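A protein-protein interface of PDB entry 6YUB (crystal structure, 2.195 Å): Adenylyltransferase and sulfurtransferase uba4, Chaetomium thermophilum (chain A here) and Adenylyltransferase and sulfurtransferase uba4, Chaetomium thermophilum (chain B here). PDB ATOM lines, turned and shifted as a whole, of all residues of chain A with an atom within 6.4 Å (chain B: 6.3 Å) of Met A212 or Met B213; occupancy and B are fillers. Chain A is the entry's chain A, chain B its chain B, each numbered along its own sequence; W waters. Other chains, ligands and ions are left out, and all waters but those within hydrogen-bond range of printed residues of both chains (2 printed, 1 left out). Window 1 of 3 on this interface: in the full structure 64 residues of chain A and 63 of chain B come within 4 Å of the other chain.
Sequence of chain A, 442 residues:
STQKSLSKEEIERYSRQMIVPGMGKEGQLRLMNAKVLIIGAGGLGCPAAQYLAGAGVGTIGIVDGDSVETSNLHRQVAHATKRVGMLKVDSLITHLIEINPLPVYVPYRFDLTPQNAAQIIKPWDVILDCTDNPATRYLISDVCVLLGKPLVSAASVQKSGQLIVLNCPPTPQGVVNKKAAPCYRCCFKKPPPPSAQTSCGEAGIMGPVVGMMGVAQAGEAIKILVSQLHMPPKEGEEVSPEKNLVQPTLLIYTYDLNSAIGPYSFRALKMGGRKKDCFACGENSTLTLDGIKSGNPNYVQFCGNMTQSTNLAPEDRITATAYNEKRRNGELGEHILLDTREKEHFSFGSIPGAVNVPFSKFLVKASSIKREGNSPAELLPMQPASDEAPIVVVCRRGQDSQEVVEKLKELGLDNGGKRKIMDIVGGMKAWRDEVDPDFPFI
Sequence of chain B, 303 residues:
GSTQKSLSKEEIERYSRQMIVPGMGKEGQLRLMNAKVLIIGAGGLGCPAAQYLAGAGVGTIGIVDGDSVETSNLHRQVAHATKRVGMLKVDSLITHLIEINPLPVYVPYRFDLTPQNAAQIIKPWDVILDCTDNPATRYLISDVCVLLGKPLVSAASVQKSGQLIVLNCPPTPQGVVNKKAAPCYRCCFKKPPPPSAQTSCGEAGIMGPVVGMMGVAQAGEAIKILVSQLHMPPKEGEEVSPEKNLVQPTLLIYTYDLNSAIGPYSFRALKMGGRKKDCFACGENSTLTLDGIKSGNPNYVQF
O of Gly A219 sits at hydrogen-bond distance from OH of Tyr B256, at 2.9 Å.
SD of Met A212 lies close to O of Met B213 (3.6 Å).
Among the printed residues, pairs that only touch across the chains: Gly A211 with Tyr B52 (3.1 Å), Pro A208 with Val B216 (3.3 Å), Gly A207 with Tyr B52 (3.4 Å), Tyr A51 with Gly B212 (3.4 Å), Val A215 with Pro B209 (3.4 Å), Met A212 with Ala B217 (3.5 Å), Tyr A51 with Gly B208 (3.6 Å), Val A215 with Met B213 (3.6 Å), Gly A219 with Pro B209 (3.7 Å), Phe A266 with Phe B267 (3.7 Å), Met A212 with Val B216 (3.7 Å), Pro A47 with Tyr B52 (3.7 Å), Tyr A51 with Pro B48 (3.8 Å), Ala A216 with Met B213 (3.8 Å), Leu A251 with Phe B267 (3.8 Å), Pro A208 with Tyr B52 (3.9 Å) and Tyr A51 with Pro B209 (3.998 Å).
Met A212 touches just these residues of chain B: Met B213, Val B216 and Ala B217.
Met B213 touches just these residues of chain A: Met A212 (3.6 Å), Val A215 (3.6 Å) and Ala A216 (3.8 Å).
Of the printed residues of chain B, Pro A208 touches Tyr B52 (3.9 Å) and Val B216 (3.3 Å).
Printed residues of chain B within 4 Å of Gly A219: Pro B209 and Tyr B256.
Of the printed residues of chain B, Pro A47 touches Tyr B52.
The nearest residue of chain A that does not touch Met B213 is Gly A219 (5.3 Å).
Hydrophobic or aromatic side chains of chain B that line the printed part of chain A: Pro B48, Tyr B52, Pro B209, Met B213, Val B216, Ala B217, Tyr B256 and Phe B267.
Printed residues of chain A that touch a printed residue of chain B: Pro A47, Tyr A51, Gly A207, Pro A208, Gly A211, Met A212, Val A215, Ala A216, Gly A219, Leu A251 and Phe A266.
Hydrophobic or aromatic side chains of chain A that line the printed part of chain B: Pro A47, Tyr A51, Met A212, Val A215, Ala A216, Leu A251 and Phe A266.
Among the printed residues, no Asp or Glu carboxylate lies within 4 Å of a Lys or Arg side-chain nitrogen of the other chain.
Water W1 lies within hydrogen-bond range of OH of Tyr A253 (2.6 Å) and O of Ala B217 (3.2 Å).
Water W2 bridges the side-chain hydroxyl (OH) of Tyr A51 (2.7 Å) and the backbone NH (N) of Gly B212 (3.4 Å).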
ATOM      1  N   LEU A  44      -7.935  23.435 -12.492  1.00  0.00           N
ATOM      2  CA  LEU A  44      -8.742  22.970 -11.373  1.00  0.00           C
ATOM      3  C   LEU A  44      -8.032  23.200 -10.045  1.00  0.00           C
ATOM      4  O   LEU A  44      -8.671  23.559  -9.049  1.00  0.00           O
ATOM      5  CB  LEU A  44      -9.067  21.487 -11.545  1.00  0.00           C
ATOM      6  CG  LEU A  44     -10.032  21.117 -12.671  1.00  0.00           C
ATOM      7  CD1 LEU A  44      -9.972  19.614 -12.953  1.00  0.00           C
ATOM      8  CD2 LEU A  44     -11.455  21.545 -12.332  1.00  0.00           C
ATOM      9  N   PRO A  47      -7.929  27.353  -8.292  1.00  0.00           N
ATOM     10  CA  PRO A  47      -9.078  27.791  -7.480  1.00  0.00           C
ATOM     11  C   PRO A  47      -9.304  26.914  -6.259  1.00  0.00           C
ATOM     12  O   PRO A  47      -9.552  27.439  -5.166  1.00  0.00           O
ATOM     13  CB  PRO A  47     -10.252  27.730  -8.472  1.00  0.00           C
ATOM     14  CG  PRO A  47      -9.797  26.804  -9.568  1.00  0.00           C
ATOM     15  CD  PRO A  47      -8.314  27.018  -9.676  1.00  0.00           C
ATOM     16  N   TYR A  51      -9.119  28.592  -2.158  1.00  0.00           N
ATOM     17  CA  TYR A  51     -10.185  28.641  -1.165  1.00  0.00           C
ATOM     18  C   TYR A  51      -9.960  27.691   0.000  1.00  0.00           C
ATOM     19  O   TYR A  51     -10.485  27.943   1.090  1.00  0.00           O
ATOM     20  CB  TYR A  51     -11.526  28.361  -1.847  1.00  0.00           C
ATOM     21  CG  TYR A  51     -11.973  29.527  -2.697  1.00  0.00           C
ATOM     22  CD1 TYR A  51     -12.714  30.568  -2.142  1.00  0.00           C
ATOM     23  CD2 TYR A  51     -11.633  29.608  -4.041  1.00  0.00           C
ATOM     24  CE1 TYR A  51     -13.115  31.645  -2.906  1.00  0.00           C
ATOM     25  CE2 TYR A  51     -12.030  30.683  -4.814  1.00  0.00           C
ATOM     26  CZ  TYR A  51     -12.770  31.704  -4.235  1.00  0.00           C
ATOM     27  OH  TYR A  51     -13.165  32.777  -4.995  1.00  0.00           O
ATOM     28  N   GLY A 207     -11.914  29.487 -19.041  1.00  0.00           N
ATOM     29  CA  GLY A 207     -11.513  29.660 -17.664  1.00  0.00           C
ATOM     30  C   GLY A 207     -12.638  29.478 -16.665  1.00  0.00           C
ATOM     31  O   GLY A 207     -12.506  28.755 -15.671  1.00  0.00           O
ATOM     32  N   PRO A 208     -13.766  30.154 -16.898  1.00  0.00           N
ATOM     33  CA  PRO A 208     -14.891  30.014 -15.951  1.00  0.00           C
ATOM     34  C   PRO A 208     -15.315  28.575 -15.722  1.00  0.00           C
ATOM     35  O   PRO A 208     -15.685  28.214 -14.599  1.00  0.00           O
ATOM     36  CB  PRO A 208     -16.004  30.848 -16.604  1.00  0.00           C
ATOM     37  CG  PRO A 208     -15.283  31.854 -17.446  1.00  0.00           C
ATOM     38  CD  PRO A 208     -14.047  31.135 -17.963  1.00  0.00           C
ATOM     39  N   VAL A 209     -15.268  27.733 -16.758  1.00  0.00           N
ATOM     40  CA  VAL A 209     -15.730  26.353 -16.612  1.00  0.00           C
ATOM     41  C   VAL A 209     -14.857  25.614 -15.606  1.00  0.00           C
ATOM     42  O   VAL A 209     -15.345  25.060 -14.615  1.00  0.00           O
ATOM     43  CB  VAL A 209     -15.742  25.640 -17.975  1.00  0.00           C
ATOM     44  CG1 VAL A 209     -16.402  24.268 -17.853  1.00  0.00           C
ATOM     45  CG2 VAL A 209     -16.457  26.476 -19.022  1.00  0.00           C
ATOM     46  N   VAL A 210     -13.542  25.596 -15.851  1.00  0.00           N
ATOM     47  CA  VAL A 210     -12.634  24.886 -14.954  1.00  0.00           C
ATOM     48  C   VAL A 210     -12.563  25.590 -13.603  1.00  0.00           C
ATOM     49  O   VAL A 210     -12.457  24.941 -12.554  1.00  0.00           O
ATOM     50  CB  VAL A 210     -11.248  24.750 -15.612  1.00  0.00           C
ATOM     51  CG1 VAL A 210     -10.463  26.055 -15.507  1.00  0.00           C
ATOM     52  CG2 VAL A 210     -10.478  23.596 -14.993  1.00  0.00           C
ATOM     53  N   GLY A 211     -12.630  26.923 -13.600  1.00  0.00           N
ATOM     54  CA  GLY A 211     -12.658  27.644 -12.339  1.00  0.00           C
ATOM     55  C   GLY A 211     -13.863  27.288 -11.491  1.00  0.00           C
ATOM     56  O   GLY A 211     -13.755  27.142 -10.270  1.00  0.00           O
ATOM     57  N   MET A 212     -15.031  27.139 -12.130  1.00  0.00           N
ATOM     58  CA  MET A 212     -16.235  26.760 -11.400  1.00  0.00           C
ATOM     59  C   MET A 212     -16.043  25.436 -10.674  1.00  0.00           C
ATOM     60  O   MET A 212     -16.269  25.341  -9.463  1.00  0.00           O
ATOM     61  CB  MET A 212     -17.418  26.667 -12.365  1.00  0.00           C
ATOM     62  CG  MET A 212     -18.755  26.461 -11.681  1.00  0.00           C
ATOM     63  SD  MET A 212     -19.388  27.995 -10.980  1.00  0.00           S
ATOM     64  CE  MET A 212     -19.711  28.913 -12.488  1.00  0.00           C
ATOM     65  N   MET A 213     -15.633  24.392 -11.406  1.00  0.00           N
ATOM     66  CA  MET A 213     -15.481  23.081 -10.789  1.00  0.00           C
ATOM     67  C   MET A 213     -14.413  23.104  -9.704  1.00  0.00           C
ATOM     68  O   MET A 213     -14.551  22.413  -8.685  1.00  0.00           O
ATOM     69  CB  MET A 213     -15.141  22.034 -11.852  1.00  0.00           C
ATOM     70  CG  MET A 213     -16.060  22.028 -13.072  1.00  0.00           C
ATOM     71  SD  MET A 213     -17.831  22.137 -12.710  1.00  0.00           S
ATOM     72  CE  MET A 213     -18.041  20.796 -11.564  1.00  0.00           C
ATOM     73  N   GLY A 214     -13.354  23.894  -9.892  1.00  0.00           N
ATOM     74  CA  GLY A 214     -12.303  23.956  -8.890  1.00  0.00           C
ATOM     75  C   GLY A 214     -12.782  24.545  -7.576  1.00  0.00           C
ATOM     76  O   GLY A 214     -12.475  24.023  -6.500  1.00  0.00           O
ATOM     77  N   VAL A 215     -13.537  25.644  -7.644  1.00  0.00           N
ATOM     78  CA  VAL A 215     -14.096  26.225  -6.427  1.00  0.00           C
ATOM     79  C   VAL A 215     -15.052  25.240  -5.766  1.00  0.00           C
ATOM     80  O   VAL A 215     -15.095  25.126  -4.533  1.00  0.00           O
ATOM     81  CB  VAL A 215     -14.797  27.561  -6.740  1.00  0.00           C
ATOM     82  CG1 VAL A 215     -15.529  28.083  -5.506  1.00  0.00           C
ATOM     83  CG2 VAL A 215     -13.790  28.584  -7.239  1.00  0.00           C
ATOM     84  N   ALA A 216     -15.849  24.534  -6.570  1.00  0.00           N
ATOM     85  CA  ALA A 216     -16.777  23.553  -6.016  1.00  0.00           C
ATOM     86  C   ALA A 216     -16.036  22.415  -5.325  1.00  0.00           C
ATOM     87  O   ALA A 216     -16.531  21.872  -4.328  1.00  0.00           O
ATOM     88  CB  ALA A 216     -17.684  23.007  -7.120  1.00  0.00           C
ATOM     89  N   GLN A 217     -14.855  22.043  -5.830  1.00  0.00           N
ATOM     90  CA  GLN A 217     -14.051  21.021  -5.168  1.00  0.00           C
ATOM     91  C   GLN A 217     -13.683  21.449  -3.752  1.00  0.00           C
ATOM     92  O   GLN A 217     -13.879  20.694  -2.793  1.00  0.00           O
ATOM     93  CB  GLN A 217     -12.786  20.734  -5.980  1.00  0.00           C
ATOM     94  CG  GLN A 217     -12.996  19.811  -7.162  1.00  0.00           C
ATOM     95  CD  GLN A 217     -11.693  19.449  -7.854  1.00  0.00           C
ATOM     96  OE1 GLN A 217     -11.186  20.208  -8.682  1.00  0.00           O
ATOM     97  NE2 GLN A 217     -11.148  18.283  -7.522  1.00  0.00           N
ATOM     98  N   GLY A 219     -15.191  23.567  -1.928  1.00  0.00           N
ATOM     99  CA  GLY A 219     -16.425  23.543  -1.157  1.00  0.00           C
ATOM    100  C   GLY A 219     -16.738  22.176  -0.582  1.00  0.00           C
ATOM    101  O   GLY A 219     -17.078  22.047   0.598  1.00  0.00           O
ATOM    102  N   GLU A 220     -16.628  21.133  -1.405  1.00  0.00           N
ATOM    103  CA  GLU A 220     -16.922  19.789  -0.918  1.00  0.00           C
ATOM    104  C   GLU A 220     -15.909  19.353   0.132  1.00  0.00           C
ATOM    105  O   GLU A 220     -16.289  18.785   1.165  1.00  0.00           O
ATOM    106  CB  GLU A 220     -16.951  18.799  -2.084  1.00  0.00           C
ATOM    107  CG  GLU A 220     -17.974  19.137  -3.148  1.00  0.00           C
ATOM    108  CD  GLU A 220     -19.368  19.306  -2.576  1.00  0.00           C
ATOM    109  OE1 GLU A 220     -19.965  18.294  -2.157  1.00  0.00           O
ATOM    110  OE2 GLU A 220     -19.855  20.455  -2.529  1.00  0.00           O
ATOM    111  N   LEU A 251     -22.305  16.439 -10.606  1.00  0.00           N
ATOM    112  CA  LEU A 251     -22.587  17.794 -11.054  1.00  0.00           C
ATOM    113  C   LEU A 251     -21.983  18.001 -12.435  1.00  0.00           C
ATOM    114  O   LEU A 251     -20.830  17.630 -12.679  1.00  0.00           O
ATOM    115  CB  LEU A 251     -22.026  18.810 -10.065  1.00  0.00           C
ATOM    116  CG  LEU A 251     -22.388  20.272 -10.328  1.00  0.00           C
ATOM    117  CD1 LEU A 251     -23.892  20.482 -10.238  1.00  0.00           C
ATOM    118  CD2 LEU A 251     -21.654  21.179  -9.351  1.00  0.00           C
ATOM    119  N   TYR A 253     -21.625  21.118 -15.295  1.00  0.00           N
ATOM    120  CA  TYR A 253     -21.777  22.534 -15.617  1.00  0.00           C
ATOM    121  C   TYR A 253     -21.569  22.690 -17.118  1.00  0.00           C
ATOM    122  O   TYR A 253     -20.448  22.535 -17.615  1.00  0.00           O
ATOM    123  CB  TYR A 253     -20.792  23.376 -14.811  1.00  0.00           C
ATOM    124  CG  TYR A 253     -20.757  24.836 -15.192  1.00  0.00           C
ATOM    125  CD1 TYR A 253     -21.916  25.599 -15.216  1.00  0.00           C
ATOM    126  CD2 TYR A 253     -19.556  25.459 -15.511  1.00  0.00           C
ATOM    127  CE1 TYR A 253     -21.883  26.937 -15.561  1.00  0.00           C
ATOM    128  CE2 TYR A 253     -19.512  26.794 -15.854  1.00  0.00           C
ATOM    129  CZ  TYR A 253     -20.678  27.529 -15.878  1.00  0.00           C
ATOM    130  OH  TYR A 253     -20.638  28.859 -16.219  1.00  0.00           O
ATOM    131  N   PHE A 266     -26.579  23.989 -14.803  1.00  0.00           N
ATOM    132  CA  PHE A 266     -26.122  23.154 -13.697  1.00  0.00           C
ATOM    133  C   PHE A 266     -27.060  21.958 -13.602  1.00  0.00           C
ATOM    134  O   PHE A 266     -28.210  22.098 -13.171  1.00  0.00           O
ATOM    135  CB  PHE A 266     -26.102  23.933 -12.387  1.00  0.00           C
ATOM    136  CG  PHE A 266     -25.025  24.977 -12.320  1.00  0.00           C
ATOM    137  CD1 PHE A 266     -23.755  24.649 -11.872  1.00  0.00           C
ATOM    138  CD2 PHE A 266     -25.278  26.278 -12.707  1.00  0.00           C
ATOM    139  CE1 PHE A 266     -22.758  25.608 -11.808  1.00  0.00           C
ATOM    140  CE2 PHE A 266     -24.290  27.239 -12.647  1.00  0.00           C
ATOM    141  CZ  PHE A 266     -23.027  26.903 -12.199  1.00  0.00           C
ATOM    142  N   PRO B  48     -13.099  36.822  -7.734  1.00  0.00           N
ATOM    143  CA  PRO B  48     -13.111  35.768  -8.761  1.00  0.00           C
ATOM    144  C   PRO B  48     -13.597  36.255 -10.114  1.00  0.00           C
ATOM    145  O   PRO B  48     -13.062  35.841 -11.150  1.00  0.00           O
ATOM    146  CB  PRO B  48     -14.044  34.700  -8.160  1.00  0.00           C
ATOM    147  CG  PRO B  48     -14.845  35.420  -7.113  1.00  0.00           C
ATOM    148  CD  PRO B  48     -13.935  36.483  -6.568  1.00  0.00           C
ATOM    149  N   TYR B  52     -11.027  36.036 -13.692  1.00  0.00           N
ATOM    150  CA  TYR B  52     -11.284  35.266 -14.906  1.00  0.00           C
ATOM    151  C   TYR B  52     -11.574  36.153 -16.106  1.00  0.00           C
ATOM    152  O   TYR B  52     -11.318  35.740 -17.245  1.00  0.00           O
ATOM    153  CB  TYR B  52     -12.426  34.284 -14.648  1.00  0.00           C
ATOM    154  CG  TYR B  52     -11.985  33.116 -13.797  1.00  0.00           C
ATOM    155  CD1 TYR B  52     -11.394  31.994 -14.376  1.00  0.00           C
ATOM    156  CD2 TYR B  52     -12.122  33.145 -12.418  1.00  0.00           C
ATOM    157  CE1 TYR B  52     -10.975  30.929 -13.604  1.00  0.00           C
ATOM    158  CE2 TYR B  52     -11.704  32.087 -11.638  1.00  0.00           C
ATOM    159  CZ  TYR B  52     -11.129  30.982 -12.236  1.00  0.00           C
ATOM    160  OH  TYR B  52     -10.715  29.931 -11.455  1.00  0.00           O
ATOM    161  N   LEU B 164     -27.621  34.504  -8.725  1.00  0.00           N
ATOM    162  CA  LEU B 164     -27.101  35.139  -9.927  1.00  0.00           C
ATOM    163  C   LEU B 164     -28.225  35.285 -10.938  1.00  0.00           C
ATOM    164  O   LEU B 164     -29.071  34.395 -11.068  1.00  0.00           O
ATOM    165  CB  LEU B 164     -25.950  34.326 -10.532  1.00  0.00           C
ATOM    166  CG  LEU B 164     -25.428  34.794 -11.890  1.00  0.00           C
ATOM    167  CD1 LEU B 164     -23.910  34.856 -11.878  1.00  0.00           C
ATOM    168  CD2 LEU B 164     -25.907  33.857 -12.981  1.00  0.00           C
ATOM    169  N   GLY B 208     -16.482  30.928   1.595  1.00  0.00           N
ATOM    170  CA  GLY B 208     -15.737  31.336   0.431  1.00  0.00           C
ATOM    171  C   GLY B 208     -16.217  30.689  -0.851  1.00  0.00           C
ATOM    172  O   GLY B 208     -16.502  31.366  -1.844  1.00  0.00           O
ATOM    173  N   PRO B 209     -16.303  29.357  -0.864  1.00  0.00           N
ATOM    174  CA  PRO B 209     -16.730  28.679  -2.102  1.00  0.00           C
ATOM    175  C   PRO B 209     -18.074  29.164  -2.624  1.00  0.00           C
ATOM    176  O   PRO B 209     -18.267  29.241  -3.844  1.00  0.00           O
ATOM    177  CB  PRO B 209     -16.774  27.196  -1.692  1.00  0.00           C
ATOM    178  CG  PRO B 209     -15.812  27.091  -0.554  1.00  0.00           C
ATOM    179  CD  PRO B 209     -15.917  28.402   0.194  1.00  0.00           C
ATOM    180  N   VAL B 210     -19.012  29.494  -1.735  1.00  0.00           N
ATOM    181  CA  VAL B 210     -20.312  29.994  -2.178  1.00  0.00           C
ATOM    182  C   VAL B 210     -20.135  31.262  -3.004  1.00  0.00           C
ATOM    183  O   VAL B 210     -20.471  31.309  -4.194  1.00  0.00           O
ATOM    184  CB  VAL B 210     -21.237  30.238  -0.972  1.00  0.00           C
ATOM    185  CG1 VAL B 210     -22.488  30.984  -1.408  1.00  0.00           C
ATOM    186  CG2 VAL B 210     -21.593  28.921  -0.295  1.00  0.00           C
ATOM    187  N   VAL B 211     -19.596  32.313  -2.379  1.00  0.00           N
ATOM    188  CA  VAL B 211     -19.417  33.580  -3.076  1.00  0.00           C
ATOM    189  C   VAL B 211     -18.426  33.429  -4.222  1.00  0.00           C
ATOM    190  O   VAL B 211     -18.533  34.117  -5.245  1.00  0.00           O
ATOM    191  CB  VAL B 211     -18.973  34.669  -2.079  1.00  0.00           C
ATOM    192  CG1 VAL B 211     -17.496  34.510  -1.728  1.00  0.00           C
ATOM    193  CG2 VAL B 211     -19.253  36.040  -2.649  1.00  0.00           C
ATOM    194  N   GLY B 212     -17.450  32.532  -4.078  1.00  0.00           N
ATOM    195  CA  GLY B 212     -16.513  32.299  -5.162  1.00  0.00           C
ATOM    196  C   GLY B 212     -17.176  31.720  -6.397  1.00  0.00           C
ATOM    197  O   GLY B 212     -16.860  32.110  -7.524  1.00  0.00           O
ATOM    198  N   MET B 213     -18.110  30.784  -6.203  1.00  0.00           N
ATOM    199  CA  MET B 213     -18.780  30.164  -7.340  1.00  0.00           C
ATOM    200  C   MET B 213     -19.663  31.162  -8.077  1.00  0.00           C
ATOM    201  O   MET B 213     -19.718  31.154  -9.312  1.00  0.00           O
ATOM    202  CB  MET B 213     -19.604  28.960  -6.876  1.00  0.00           C
ATOM    203  CG  MET B 213     -18.843  27.641  -6.965  1.00  0.00           C
ATOM    204  SD  MET B 213     -19.801  26.186  -6.517  1.00  0.00           S
ATOM    205  CE  MET B 213     -19.392  26.021  -4.780  1.00  0.00           C
ATOM    206  N   MET B 214     -20.366  32.027  -7.341  1.00  0.00           N
ATOM    207  CA  MET B 214     -21.194  33.034  -7.993  1.00  0.00           C
ATOM    208  C   MET B 214     -20.332  34.012  -8.782  1.00  0.00           C
ATOM    209  O   MET B 214     -20.683  34.404  -9.901  1.00  0.00           O
ATOM    210  CB  MET B 214     -22.037  33.778  -6.963  1.00  0.00           C
ATOM    211  CG  MET B 214     -22.888  32.886  -6.071  1.00  0.00           C
ATOM    212  SD  MET B 214     -23.820  31.613  -6.946  1.00  0.00           S
ATOM    213  CE  MET B 214     -24.746  32.572  -8.119  1.00  0.00           C
ATOM    214  N   GLY B 215     -19.189  34.412  -8.218  1.00  0.00           N
ATOM    215  CA  GLY B 215     -18.312  35.331  -8.925  1.00  0.00           C
ATOM    216  C   GLY B 215     -17.787  34.750 -10.223  1.00  0.00           C
ATOM    217  O   GLY B 215     -17.806  35.409 -11.267  1.00  0.00           O
ATOM    218  N   VAL B 216     -17.300  33.509 -10.173  1.00  0.00           N
ATOM    219  CA  VAL B 216     -16.863  32.845 -11.397  1.00  0.00           C
ATOM    220  C   VAL B 216     -18.008  32.778 -12.396  1.00  0.00           C
ATOM    221  O   VAL B 216     -17.833  33.061 -13.587  1.00  0.00           O
ATOM    222  CB  VAL B 216     -16.302  31.446 -11.077  1.00  0.00           C
ATOM    223  CG1 VAL B 216     -16.069  30.657 -12.359  1.00  0.00           C
ATOM    224  CG2 VAL B 216     -15.011  31.562 -10.279  1.00  0.00           C
ATOM    225  N   ALA B 217     -19.207  32.422 -11.925  1.00  0.00           N
ATOM    226  CA  ALA B 217     -20.371  32.386 -12.803  1.00  0.00           C
ATOM    227  C   ALA B 217     -20.642  33.753 -13.425  1.00  0.00           C
ATOM    228  O   ALA B 217     -21.010  33.843 -14.603  1.00  0.00           O
ATOM    229  CB  ALA B 217     -21.594  31.904 -12.022  1.00  0.00           C
ATOM    230  N   GLN B 218     -20.449  34.830 -12.655  1.00  0.00           N
ATOM    231  CA  GLN B 218     -20.642  36.169 -13.199  1.00  0.00           C
ATOM    232  C   GLN B 218     -19.707  36.435 -14.370  1.00  0.00           C
ATOM    233  O   GLN B 218     -20.122  37.010 -15.386  1.00  0.00           O
ATOM    234  CB  GLN B 218     -20.407  37.216 -12.113  1.00  0.00           C
ATOM    235  CG  GLN B 218     -21.609  37.583 -11.304  1.00  0.00           C
ATOM    236  CD  GLN B 218     -21.291  38.665 -10.288  1.00  0.00           C
ATOM    237  OE1 GLN B 218     -20.569  38.427  -9.322  1.00  0.00           O
ATOM    238  NE2 GLN B 218     -21.822  39.859 -10.511  1.00  0.00           N
ATOM    239  N   TYR B 254     -27.796  28.812  -5.525  1.00  0.00           N
ATOM    240  CA  TYR B 254     -26.940  27.737  -5.042  1.00  0.00           C
ATOM    241  C   TYR B 254     -26.986  27.715  -3.521  1.00  0.00           C
ATOM    242  O   TYR B 254     -26.579  28.683  -2.871  1.00  0.00           O
ATOM    243  CB  TYR B 254     -25.505  27.911  -5.533  1.00  0.00           C
ATOM    244  CG  TYR B 254     -24.556  26.897  -4.936  1.00  0.00           C
ATOM    245  CD1 TYR B 254     -24.854  25.540  -4.970  1.00  0.00           C
ATOM    246  CD2 TYR B 254     -23.371  27.293  -4.336  1.00  0.00           C
ATOM    247  CE1 TYR B 254     -24.001  24.608  -4.421  1.00  0.00           C
ATOM    248  CE2 TYR B 254     -22.505  26.366  -3.785  1.00  0.00           C
ATOM    249  CZ  TYR B 254     -22.824  25.028  -3.831  1.00  0.00           C
ATOM    250  OH  TYR B 254     -21.975  24.099  -3.285  1.00  0.00           O
ATOM    251  N   TYR B 256     -25.766  26.010   0.021  1.00  0.00           N
ATOM    252  CA  TYR B 256     -24.560  25.362   0.538  1.00  0.00           C
ATOM    253  C   TYR B 256     -24.805  25.001   1.997  1.00  0.00           C
ATOM    254  O   TYR B 256     -24.961  25.888   2.844  1.00  0.00           O
ATOM    255  CB  TYR B 256     -23.357  26.289   0.386  1.00  0.00           C
ATOM    256  CG  TYR B 256     -22.024  25.715   0.821  1.00  0.00           C
ATOM    257  CD1 TYR B 256     -21.615  25.779   2.147  1.00  0.00           C
ATOM    258  CD2 TYR B 256     -21.164  25.138  -0.102  1.00  0.00           C
ATOM    259  CE1 TYR B 256     -20.396  25.268   2.543  1.00  0.00           C
ATOM    260  CE2 TYR B 256     -19.943  24.625   0.283  1.00  0.00           C
ATOM    261  CZ  TYR B 256     -19.561  24.693   1.609  1.00  0.00           C
ATOM    262  OH  TYR B 256     -18.338  24.186   2.003  1.00  0.00           O
ATOM    263  N   PHE B 267     -28.525  23.352  -6.580  1.00  0.00           N
ATOM    264  CA  PHE B 267     -28.696  24.390  -7.588  1.00  0.00           C
ATOM    265  C   PHE B 267     -30.160  24.413  -8.025  1.00  0.00           C
ATOM    266  O   PHE B 267     -30.686  23.397  -8.483  1.00  0.00           O
ATOM    267  CB  PHE B 267     -27.795  24.138  -8.797  1.00  0.00           C
ATOM    268  CG  PHE B 267     -26.347  24.422  -8.549  1.00  0.00           C
ATOM    269  CD1 PHE B 267     -25.836  25.694  -8.747  1.00  0.00           C
ATOM    270  CD2 PHE B 267     -25.491  23.422  -8.126  1.00  0.00           C
ATOM    271  CE1 PHE B 267     -24.497  25.965  -8.526  1.00  0.00           C
ATOM    272  CE2 PHE B 267     -24.150  23.685  -7.900  1.00  0.00           C
ATOM    273  CZ  PHE B 267     -23.654  24.955  -8.103  1.00  0.00           C
HETATM  274  O   HOH W   1     -21.859  31.199 -16.108  1.00  0.00           O
HETATM  275  O   HOH W   2     -14.672  34.386  -3.474  1.00  0.00           O
